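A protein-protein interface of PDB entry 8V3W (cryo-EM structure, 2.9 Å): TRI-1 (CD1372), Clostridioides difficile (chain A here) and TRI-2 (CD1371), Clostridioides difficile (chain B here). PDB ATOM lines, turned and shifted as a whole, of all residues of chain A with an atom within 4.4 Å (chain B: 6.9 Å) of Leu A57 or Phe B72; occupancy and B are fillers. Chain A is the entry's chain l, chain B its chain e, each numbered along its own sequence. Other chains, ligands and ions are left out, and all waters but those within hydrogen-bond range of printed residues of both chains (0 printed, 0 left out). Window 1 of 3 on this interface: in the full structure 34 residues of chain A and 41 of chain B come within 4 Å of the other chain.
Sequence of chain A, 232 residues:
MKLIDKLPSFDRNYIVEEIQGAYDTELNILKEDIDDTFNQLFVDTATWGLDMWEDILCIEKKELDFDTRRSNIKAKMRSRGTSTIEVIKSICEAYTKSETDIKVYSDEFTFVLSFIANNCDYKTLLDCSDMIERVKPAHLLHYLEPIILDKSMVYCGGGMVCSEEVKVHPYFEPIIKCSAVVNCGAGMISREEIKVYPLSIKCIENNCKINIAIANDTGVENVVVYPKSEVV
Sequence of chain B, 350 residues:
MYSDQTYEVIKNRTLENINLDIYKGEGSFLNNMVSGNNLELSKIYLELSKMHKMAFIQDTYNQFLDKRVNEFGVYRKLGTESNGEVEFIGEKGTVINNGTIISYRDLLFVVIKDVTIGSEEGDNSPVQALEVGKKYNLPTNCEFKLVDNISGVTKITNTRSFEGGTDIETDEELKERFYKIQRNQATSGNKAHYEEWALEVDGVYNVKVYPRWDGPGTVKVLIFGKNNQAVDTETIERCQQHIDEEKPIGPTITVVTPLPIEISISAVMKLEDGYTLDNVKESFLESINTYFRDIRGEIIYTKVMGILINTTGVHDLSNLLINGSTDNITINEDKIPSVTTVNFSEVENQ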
ATOM      1  N   TRP A  53      31.852  14.157 -26.416  1.00  0.00           N
ATOM      2  CA  TRP A  53      31.307  13.358 -25.326  1.00  0.00           C
ATOM      3  C   TRP A  53      31.194  14.162 -24.037  1.00  0.00           C
ATOM      4  O   TRP A  53      30.311  13.888 -23.214  1.00  0.00           O
ATOM      5  CB  TRP A  53      32.180  12.133 -25.070  1.00  0.00           C
ATOM      6  CG  TRP A  53      32.228  11.107 -26.155  1.00  0.00           C
ATOM      7  CD1 TRP A  53      33.028  11.117 -27.258  1.00  0.00           C
ATOM      8  CD2 TRP A  53      31.482   9.886 -26.213  1.00  0.00           C
ATOM      9  NE1 TRP A  53      32.811   9.989 -28.010  1.00  0.00           N
ATOM     10  CE2 TRP A  53      31.868   9.217 -27.388  1.00  0.00           C
ATOM     11  CE3 TRP A  53      30.517   9.300 -25.389  1.00  0.00           C
ATOM     12  CZ2 TRP A  53      31.316   7.996 -27.767  1.00  0.00           C
ATOM     13  CZ3 TRP A  53      29.974   8.087 -25.762  1.00  0.00           C
ATOM     14  CH2 TRP A  53      30.376   7.446 -26.940  1.00  0.00           C
ATOM     15  N   GLU A  54      32.094  15.127 -23.831  1.00  0.00           N
ATOM     16  CA  GLU A  54      32.039  15.962 -22.635  1.00  0.00           C
ATOM     17  C   GLU A  54      30.715  16.701 -22.533  1.00  0.00           C
ATOM     18  O   GLU A  54      30.219  16.937 -21.424  1.00  0.00           O
ATOM     19  CB  GLU A  54      33.205  16.955 -22.639  1.00  0.00           C
ATOM     20  CG  GLU A  54      34.500  16.474 -21.977  1.00  0.00           C
ATOM     21  CD  GLU A  54      35.213  15.352 -22.722  1.00  0.00           C
ATOM     22  OE1 GLU A  54      34.579  14.652 -23.536  1.00  0.00           O
ATOM     23  OE2 GLU A  54      36.427  15.173 -22.492  1.00  0.00           O
ATOM     24  N   ASP A  55      30.129  17.074 -23.670  1.00  0.00           N
ATOM     25  CA  ASP A  55      28.827  17.726 -23.660  1.00  0.00           C
ATOM     26  C   ASP A  55      27.720  16.793 -23.189  1.00  0.00           C
ATOM     27  O   ASP A  55      26.681  17.272 -22.726  1.00  0.00           O
ATOM     28  CB  ASP A  55      28.500  18.262 -25.053  1.00  0.00           C
ATOM     29  CG  ASP A  55      29.721  18.811 -25.766  1.00  0.00           C
ATOM     30  OD1 ASP A  55      30.540  19.487 -25.108  1.00  0.00           O
ATOM     31  OD2 ASP A  55      29.861  18.566 -26.982  1.00  0.00           O
ATOM     32  N   ILE A  56      27.919  15.480 -23.292  1.00  0.00           N
ATOM     33  CA  ILE A  56      26.896  14.525 -22.886  1.00  0.00           C
ATOM     34  C   ILE A  56      27.162  13.923 -21.509  1.00  0.00           C
ATOM     35  O   ILE A  56      26.225  13.398 -20.888  1.00  0.00           O
ATOM     36  CB  ILE A  56      26.741  13.405 -23.937  1.00  0.00           C
ATOM     37  CG1 ILE A  56      25.290  12.927 -23.994  1.00  0.00           C
ATOM     38  CG2 ILE A  56      27.668  12.236 -23.639  1.00  0.00           C
ATOM     39  CD1 ILE A  56      25.049  11.859 -25.029  1.00  0.00           C
ATOM     40  N   LEU A  57      28.396  13.981 -21.014  1.00  0.00           N
ATOM     41  CA  LEU A  57      28.722  13.448 -19.697  1.00  0.00           C
ATOM     42  C   LEU A  57      29.068  14.528 -18.682  1.00  0.00           C
ATOM     43  O   LEU A  57      29.460  14.197 -17.558  1.00  0.00           O
ATOM     44  CB  LEU A  57      29.874  12.444 -19.803  1.00  0.00           C
ATOM     45  CG  LEU A  57      29.504  11.100 -20.431  1.00  0.00           C
ATOM     46  CD1 LEU A  57      30.680  10.138 -20.385  1.00  0.00           C
ATOM     47  CD2 LEU A  57      28.293  10.503 -19.736  1.00  0.00           C
ATOM     48  N   CYS A  58      28.938  15.805 -19.050  1.00  0.00           N
ATOM     49  CA  CYS A  58      29.126  16.927 -18.130  1.00  0.00           C
ATOM     50  C   CYS A  58      30.490  16.881 -17.443  1.00  0.00           C
ATOM     51  O   CYS A  58      30.623  17.211 -16.264  1.00  0.00           O
ATOM     52  CB  CYS A  58      27.998  16.985 -17.100  1.00  0.00           C
ATOM     53  SG  CYS A  58      26.385  17.406 -17.797  1.00  0.00           S
ATOM     54  N   ILE A  59      31.514  16.469 -18.189  1.00  0.00           N
ATOM     55  CA  ILE A  59      32.856  16.377 -17.620  1.00  0.00           C
ATOM     56  C   ILE A  59      33.396  17.766 -17.298  1.00  0.00           C
ATOM     57  O   ILE A  59      33.888  18.014 -16.190  1.00  0.00           O
ATOM     58  CB  ILE A  59      33.784  15.606 -18.574  1.00  0.00           C
ATOM     59  CG1 ILE A  59      33.143  14.275 -18.973  1.00  0.00           C
ATOM     60  CG2 ILE A  59      35.132  15.367 -17.935  1.00  0.00           C
ATOM     61  CD1 ILE A  59      32.761  13.405 -17.798  1.00  0.00           C
ATOM     62  N   ILE A  73      36.061   9.375 -19.257  1.00  0.00           N
ATOM     63  CA  ILE A  73      34.768   9.077 -19.865  1.00  0.00           C
ATOM     64  C   ILE A  73      34.307   7.682 -19.469  1.00  0.00           C
ATOM     65  O   ILE A  73      33.144   7.474 -19.094  1.00  0.00           O
ATOM     66  CB  ILE A  73      34.863   9.234 -21.392  1.00  0.00           C
ATOM     67  CG1 ILE A  73      35.166  10.691 -21.738  1.00  0.00           C
ATOM     68  CG2 ILE A  73      33.585   8.752 -22.055  1.00  0.00           C
ATOM     69  CD1 ILE A  73      34.663  11.126 -23.062  1.00  0.00           C
ATOM     70  N   LYS A  76      33.170   7.857 -15.766  1.00  0.00           N
ATOM     71  CA  LYS A  76      31.867   8.492 -15.613  1.00  0.00           C
ATOM     72  C   LYS A  76      30.753   7.581 -16.108  1.00  0.00           C
ATOM     73  O   LYS A  76      29.659   7.553 -15.533  1.00  0.00           O
ATOM     74  CB  LYS A  76      31.845   9.827 -16.358  1.00  0.00           C
ATOM     75  CG  LYS A  76      30.463  10.460 -16.496  1.00  0.00           C
ATOM     76  CD  LYS A  76      29.875  10.865 -15.152  1.00  0.00           C
ATOM     77  CE  LYS A  76      28.585  11.649 -15.334  1.00  0.00           C
ATOM     78  NZ  LYS A  76      27.977  12.044 -14.035  1.00  0.00           N
ATOM     79  N   ASP B  66      16.264   9.815 -27.750  1.00  0.00           N
ATOM     80  CA  ASP B  66      15.502   8.752 -27.106  1.00  0.00           C
ATOM     81  C   ASP B  66      16.349   7.498 -26.937  1.00  0.00           C
ATOM     82  O   ASP B  66      16.362   6.879 -25.867  1.00  0.00           O
ATOM     83  CB  ASP B  66      14.246   8.446 -27.920  1.00  0.00           C
ATOM     84  CG  ASP B  66      13.301   7.512 -27.201  1.00  0.00           C
ATOM     85  OD1 ASP B  66      13.264   7.552 -25.954  1.00  0.00           O
ATOM     86  OD2 ASP B  66      12.598   6.734 -27.878  1.00  0.00           O
ATOM     87  N   LYS B  67      17.079   7.114 -27.984  1.00  0.00           N
ATOM     88  CA  LYS B  67      17.901   5.913 -27.894  1.00  0.00           C
ATOM     89  C   LYS B  67      19.075   6.115 -26.944  1.00  0.00           C
ATOM     90  O   LYS B  67      19.448   5.193 -26.212  1.00  0.00           O
ATOM     91  CB  LYS B  67      18.381   5.498 -29.282  1.00  0.00           C
ATOM     92  CG  LYS B  67      17.249   5.083 -30.203  1.00  0.00           C
ATOM     93  CD  LYS B  67      17.698   4.018 -31.182  1.00  0.00           C
ATOM     94  CE  LYS B  67      16.516   3.379 -31.894  1.00  0.00           C
ATOM     95  NZ  LYS B  67      16.922   2.164 -32.652  1.00  0.00           N
ATOM     96  N   ARG B  68      19.660   7.312 -26.929  1.00  0.00           N
ATOM     97  CA  ARG B  68      20.764   7.567 -26.010  1.00  0.00           C
ATOM     98  C   ARG B  68      20.300   7.530 -24.556  1.00  0.00           C
ATOM     99  O   ARG B  68      20.997   6.988 -23.689  1.00  0.00           O
ATOM    100  CB  ARG B  68      21.422   8.907 -26.340  1.00  0.00           C
ATOM    101  CG  ARG B  68      22.941   8.857 -26.315  1.00  0.00           C
ATOM    102  CD  ARG B  68      23.552   9.665 -27.448  1.00  0.00           C
ATOM    103  NE  ARG B  68      23.742   8.883 -28.664  1.00  0.00           N
ATOM    104  CZ  ARG B  68      24.741   8.032 -28.866  1.00  0.00           C
ATOM    105  NH1 ARG B  68      25.643   7.789 -27.930  1.00  0.00           N
ATOM    106  NH2 ARG B  68      24.838   7.414 -30.040  1.00  0.00           N
ATOM    107  N   VAL B  69      19.126   8.092 -24.263  1.00  0.00           N
ATOM    108  CA  VAL B  69      18.654   8.051 -22.883  1.00  0.00           C
ATOM    109  C   VAL B  69      18.161   6.656 -22.513  1.00  0.00           C
ATOM    110  O   VAL B  69      18.201   6.277 -21.338  1.00  0.00           O
ATOM    111  CB  VAL B  69      17.573   9.117 -22.632  1.00  0.00           C
ATOM    112  CG1 VAL B  69      18.150  10.513 -22.831  1.00  0.00           C
ATOM    113  CG2 VAL B  69      16.360   8.889 -23.509  1.00  0.00           C
ATOM    114  N   ASN B  70      17.688   5.872 -23.485  1.00  0.00           N
ATOM    115  CA  ASN B  70      17.426   4.463 -23.214  1.00  0.00           C
ATOM    116  C   ASN B  70      18.717   3.715 -22.918  1.00  0.00           C
ATOM    117  O   ASN B  70      18.722   2.779 -22.111  1.00  0.00           O
ATOM    118  CB  ASN B  70      16.699   3.823 -24.395  1.00  0.00           C
ATOM    119  CG  ASN B  70      15.217   4.137 -24.407  1.00  0.00           C
ATOM    120  OD1 ASN B  70      14.765   5.085 -23.763  1.00  0.00           O
ATOM    121  ND2 ASN B  70      14.450   3.338 -25.139  1.00  0.00           N
ATOM    122  N   GLU B  71      19.811   4.103 -23.573  1.00  0.00           N
ATOM    123  CA  GLU B  71      21.123   3.576 -23.215  1.00  0.00           C
ATOM    124  C   GLU B  71      21.478   3.932 -21.781  1.00  0.00           C
ATOM    125  O   GLU B  71      21.996   3.095 -21.034  1.00  0.00           O
ATOM    126  CB  GLU B  71      22.189   4.122 -24.165  1.00  0.00           C
ATOM    127  CG  GLU B  71      22.161   3.556 -25.564  1.00  0.00           C
ATOM    128  CD  GLU B  71      23.291   4.097 -26.418  1.00  0.00           C
ATOM    129  OE1 GLU B  71      23.638   5.283 -26.251  1.00  0.00           O
ATOM    130  OE2 GLU B  71      23.837   3.340 -27.247  1.00  0.00           O
ATOM    131  N   PHE B  72      21.210   5.172 -21.380  1.00  0.00           N
ATOM    132  CA  PHE B  72      21.582   5.649 -20.055  1.00  0.00           C
ATOM    133  C   PHE B  72      20.512   5.387 -19.002  1.00  0.00           C
ATOM    134  O   PHE B  72      20.677   5.810 -17.853  1.00  0.00           O
ATOM    135  CB  PHE B  72      21.914   7.144 -20.111  1.00  0.00           C
ATOM    136  CG  PHE B  72      23.301   7.429 -20.611  1.00  0.00           C
ATOM    137  CD1 PHE B  72      23.544   7.600 -21.962  1.00  0.00           C
ATOM    138  CD2 PHE B  72      24.367   7.507 -19.730  1.00  0.00           C
ATOM    139  CE1 PHE B  72      24.821   7.852 -22.424  1.00  0.00           C
ATOM    140  CE2 PHE B  72      25.643   7.758 -20.187  1.00  0.00           C
ATOM    141  CZ  PHE B  72      25.872   7.931 -21.533  1.00  0.00           C
ATOM    142  N   GLY B  73      19.426   4.705 -19.360  1.00  0.00           N
ATOM    143  CA  GLY B  73      18.416   4.303 -18.406  1.00  0.00           C
ATOM    144  C   GLY B  73      17.273   5.275 -18.222  1.00  0.00           C
ATOM    145  O   GLY B  73      16.271   4.912 -17.592  1.00  0.00           O
ATOM    146  N   VAL B  74      17.380   6.495 -18.750  1.00  0.00           N
ATOM    147  CA  VAL B  74      16.314   7.476 -18.599  1.00  0.00           C
ATOM    148  C   VAL B  74      15.084   7.023 -19.373  1.00  0.00           C
ATOM    149  O   VAL B  74      15.186   6.454 -20.467  1.00  0.00           O
ATOM    150  CB  VAL B  74      16.791   8.859 -19.071  1.00  0.00           C
ATOM    151  CG1 VAL B  74      15.812   9.938 -18.637  1.00  0.00           C
ATOM    152  CG2 VAL B  74      18.185   9.146 -18.538  1.00  0.00           C
ATOM    153  N   TYR B  75      13.911   7.265 -18.798  1.00  0.00           N
ATOM    154  CA  TYR B  75      12.640   6.919 -19.416  1.00  0.00           C
ATOM    155  C   TYR B  75      11.730   8.135 -19.435  1.00  0.00           C
ATOM    156  O   TYR B  75      11.691   8.907 -18.473  1.00  0.00           O
ATOM    157  CB  TYR B  75      11.949   5.775 -18.669  1.00  0.00           C
ATOM    158  CG  TYR B  75      12.020   4.447 -19.379  1.00  0.00           C
ATOM    159  CD1 TYR B  75      13.227   3.953 -19.847  1.00  0.00           C
ATOM    160  CD2 TYR B  75      10.877   3.686 -19.581  1.00  0.00           C
ATOM    161  CE1 TYR B  75      13.294   2.742 -20.498  1.00  0.00           C
ATOM    162  CE2 TYR B  75      10.936   2.468 -20.231  1.00  0.00           C
ATOM    163  CZ  TYR B  75      12.150   2.001 -20.686  1.00  0.00           C
ATOM    164  OH  TYR B  75      12.225   0.791 -21.334  1.00  0.00           O
ATOM    165  N   PHE B 178      17.761  14.637 -17.908  1.00  0.00           N
ATOM    166  CA  PHE B 178      18.948  13.829 -18.163  1.00  0.00           C
ATOM    167  C   PHE B 178      20.211  14.585 -17.783  1.00  0.00           C
ATOM    168  O   PHE B 178      21.121  14.021 -17.165  1.00  0.00           O
ATOM    169  CB  PHE B 178      18.991  13.411 -19.632  1.00  0.00           C
ATOM    170  CG  PHE B 178      20.305  12.822 -20.057  1.00  0.00           C
ATOM    171  CD1 PHE B 178      20.664  11.542 -19.673  1.00  0.00           C
ATOM    172  CD2 PHE B 178      21.180  13.548 -20.847  1.00  0.00           C
ATOM    173  CE1 PHE B 178      21.873  10.998 -20.066  1.00  0.00           C
ATOM    174  CE2 PHE B 178      22.388  13.010 -21.244  1.00  0.00           C
ATOM    175  CZ  PHE B 178      22.735  11.734 -20.854  1.00  0.00           C
ATOM    176  N   TYR B 179      20.275  15.871 -18.131  1.00  0.00           N
ATOM    177  CA  TYR B 179      21.437  16.674 -17.768  1.00  0.00           C
ATOM    178  C   TYR B 179      21.583  16.787 -16.254  1.00  0.00           C
ATOM    179  O   TYR B 179      22.691  16.653 -15.716  1.00  0.00           O
ATOM    180  CB  TYR B 179      21.326  18.056 -18.410  1.00  0.00           C
ATOM    181  CG  TYR B 179      21.934  18.125 -19.791  1.00  0.00           C
ATOM    182  CD1 TYR B 179      23.308  18.227 -19.963  1.00  0.00           C
ATOM    183  CD2 TYR B 179      21.136  18.070 -20.926  1.00  0.00           C
ATOM    184  CE1 TYR B 179      23.869  18.284 -21.224  1.00  0.00           C
ATOM    185  CE2 TYR B 179      21.688  18.126 -22.190  1.00  0.00           C
ATOM    186  CZ  TYR B 179      23.053  18.233 -22.332  1.00  0.00           C
ATOM    187  OH  TYR B 179      23.604  18.290 -23.594  1.00  0.00           O
ATOM    188  N   GLN B 182      22.760  13.516 -14.824  1.00  0.00           N
ATOM    189  CA  GLN B 182      24.169  13.315 -15.137  1.00  0.00           C
ATOM    190  C   GLN B 182      25.063  14.184 -14.266  1.00  0.00           C
ATOM    191  O   GLN B 182      26.183  13.780 -13.934  1.00  0.00           O
ATOM    192  CB  GLN B 182      24.425  13.591 -16.617  1.00  0.00           C
ATOM    193  CG  GLN B 182      23.933  12.487 -17.544  1.00  0.00           C
ATOM    194  CD  GLN B 182      24.879  11.301 -17.620  1.00  0.00           C
ATOM    195  OE1 GLN B 182      25.608  11.005 -16.674  1.00  0.00           O
ATOM    196  NE2 GLN B 182      24.871  10.615 -18.756  1.00  0.00           N
ATOM    197  N   ARG B 183      24.592  15.374 -13.889  1.00  0.00           N
ATOM    198  CA  ARG B 183      25.355  16.187 -12.948  1.00  0.00           C
ATOM    199  C   ARG B 183      25.415  15.529 -11.575  1.00  0.00           C
ATOM    200  O   ARG B 183      26.433  15.623 -10.880  1.00  0.00           O
ATOM    201  CB  ARG B 183      24.752  17.587 -12.849  1.00  0.00           C
ATOM    202  CG  ARG B 183      25.788  18.692 -12.770  1.00  0.00           C
ATOM    203  CD  ARG B 183      25.282  19.986 -13.384  1.00  0.00           C
ATOM    204  NE  ARG B 183      25.025  19.855 -14.812  1.00  0.00           N
ATOM    205  CZ  ARG B 183      23.825  19.668 -15.344  1.00  0.00           C
ATOM    206  NH1 ARG B 183      22.741  19.585 -14.590  1.00  0.00           N
ATOM    207  NH2 ARG B 183      23.709  19.560 -16.665  1.00  0.00           N
ATOM    208  N   GLN B 185      25.746  12.552  -8.821  1.00  0.00           N
ATOM    209  CA  GLN B 185      26.496  11.304  -8.686  1.00  0.00           C
ATOM    210  C   GLN B 185      25.828  10.481  -7.589  1.00  0.00           C
ATOM    211  O   GLN B 185      26.115  10.666  -6.403  1.00  0.00           O
ATOM    212  CB  GLN B 185      27.966  11.571  -8.368  1.00  0.00           C
ATOM    213  CG  GLN B 185      28.764  12.165  -9.519  1.00  0.00           C
ATOM    214  CD  GLN B 185      28.460  13.632  -9.746  1.00  0.00           C
ATOM    215  OE1 GLN B 185      28.051  14.341  -8.828  1.00  0.00           O
ATOM    216  NE2 GLN B 185      28.656  14.094 -10.975  1.00  0.00           N
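Printed residues of chain B within 4 Å of Ile A56: Arg B68 (3.6 Å), Phe B178 (3.9 Å) and Gln B182 (3.8 Å). Leu A57 touches two residues of chain B. Asp B66 touches none of the printed residues of chain A. Printed residues of chain A within 4 Å of Arg B68: Ile A56. Of chain A, only Leu A57 (3.8 Å) comes within 4 Å of Phe B72. Val B74 touches none of the printed residues of chain A. Of the printed residues of chain A, Phe B178 touches Ile A56 (3.9 Å). Printed residues of chain A within 4 Å of Arg B183: Cys A58. Of the printed residues of chain A, Gln B185 touches Lys A76. The nearest residue of chain B that does not touch Leu A57 is Phe B178 (5.8 Å). The nearest printed residue of chain A that does not touch Phe B72 is Ile A56 (4.8 Å). The nearest printed residue of chain B that does not touch Lys A76 is Arg B183 (4.8 Å).
The guanidinium group of Arg B183 is in hydrogen-bond range of the backbone carbonyl oxygen of Tyr B179 (3.1 Å). O of Arg B183 sits at hydrogen-bond distance from NE2 of Gln B185 (2.7 Å). The guanidinium group of Arg B68 is in salt-bridge range of the side-chain carboxylate of Glu B71, at 3.6 Å.
Hydrophobic or aromatic side chains of chain A within 4 Å of the printed part of chain B: Ile A56 and Leu A57. Along chain A the printed residues that touch a printed residue of chain B span positions 55 to 76. Among the printed residues, 10 pairs touch across the chains. Among the printed residues, no Asp or Glu carboxylate lies within 4 Å of a Lys or Arg side-chain nitrogen of the other chain.
Among the printed residues, pairs that only touch across the chains: Ile A56 with Arg B68, Ile A56 with Phe B178, Ile A56 with Gln B182, Leu A57 with Phe B72, Leu A57 with Gln B182, Cys A58 with Tyr B179 and Lys A76 with Gln B185.
The side-chain hydroxyl of Tyr B179 sits close to the backbone carbonyl oxygen of Asp A55, 3.4 Å away. The side-chain sulfur of Cys A58 lies within hydrogen-bond range of the guanidinium group of Arg B183. NZ of Lys A76 lies within hydrogen-bond range of O of Gln B182 (2.5 Å).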
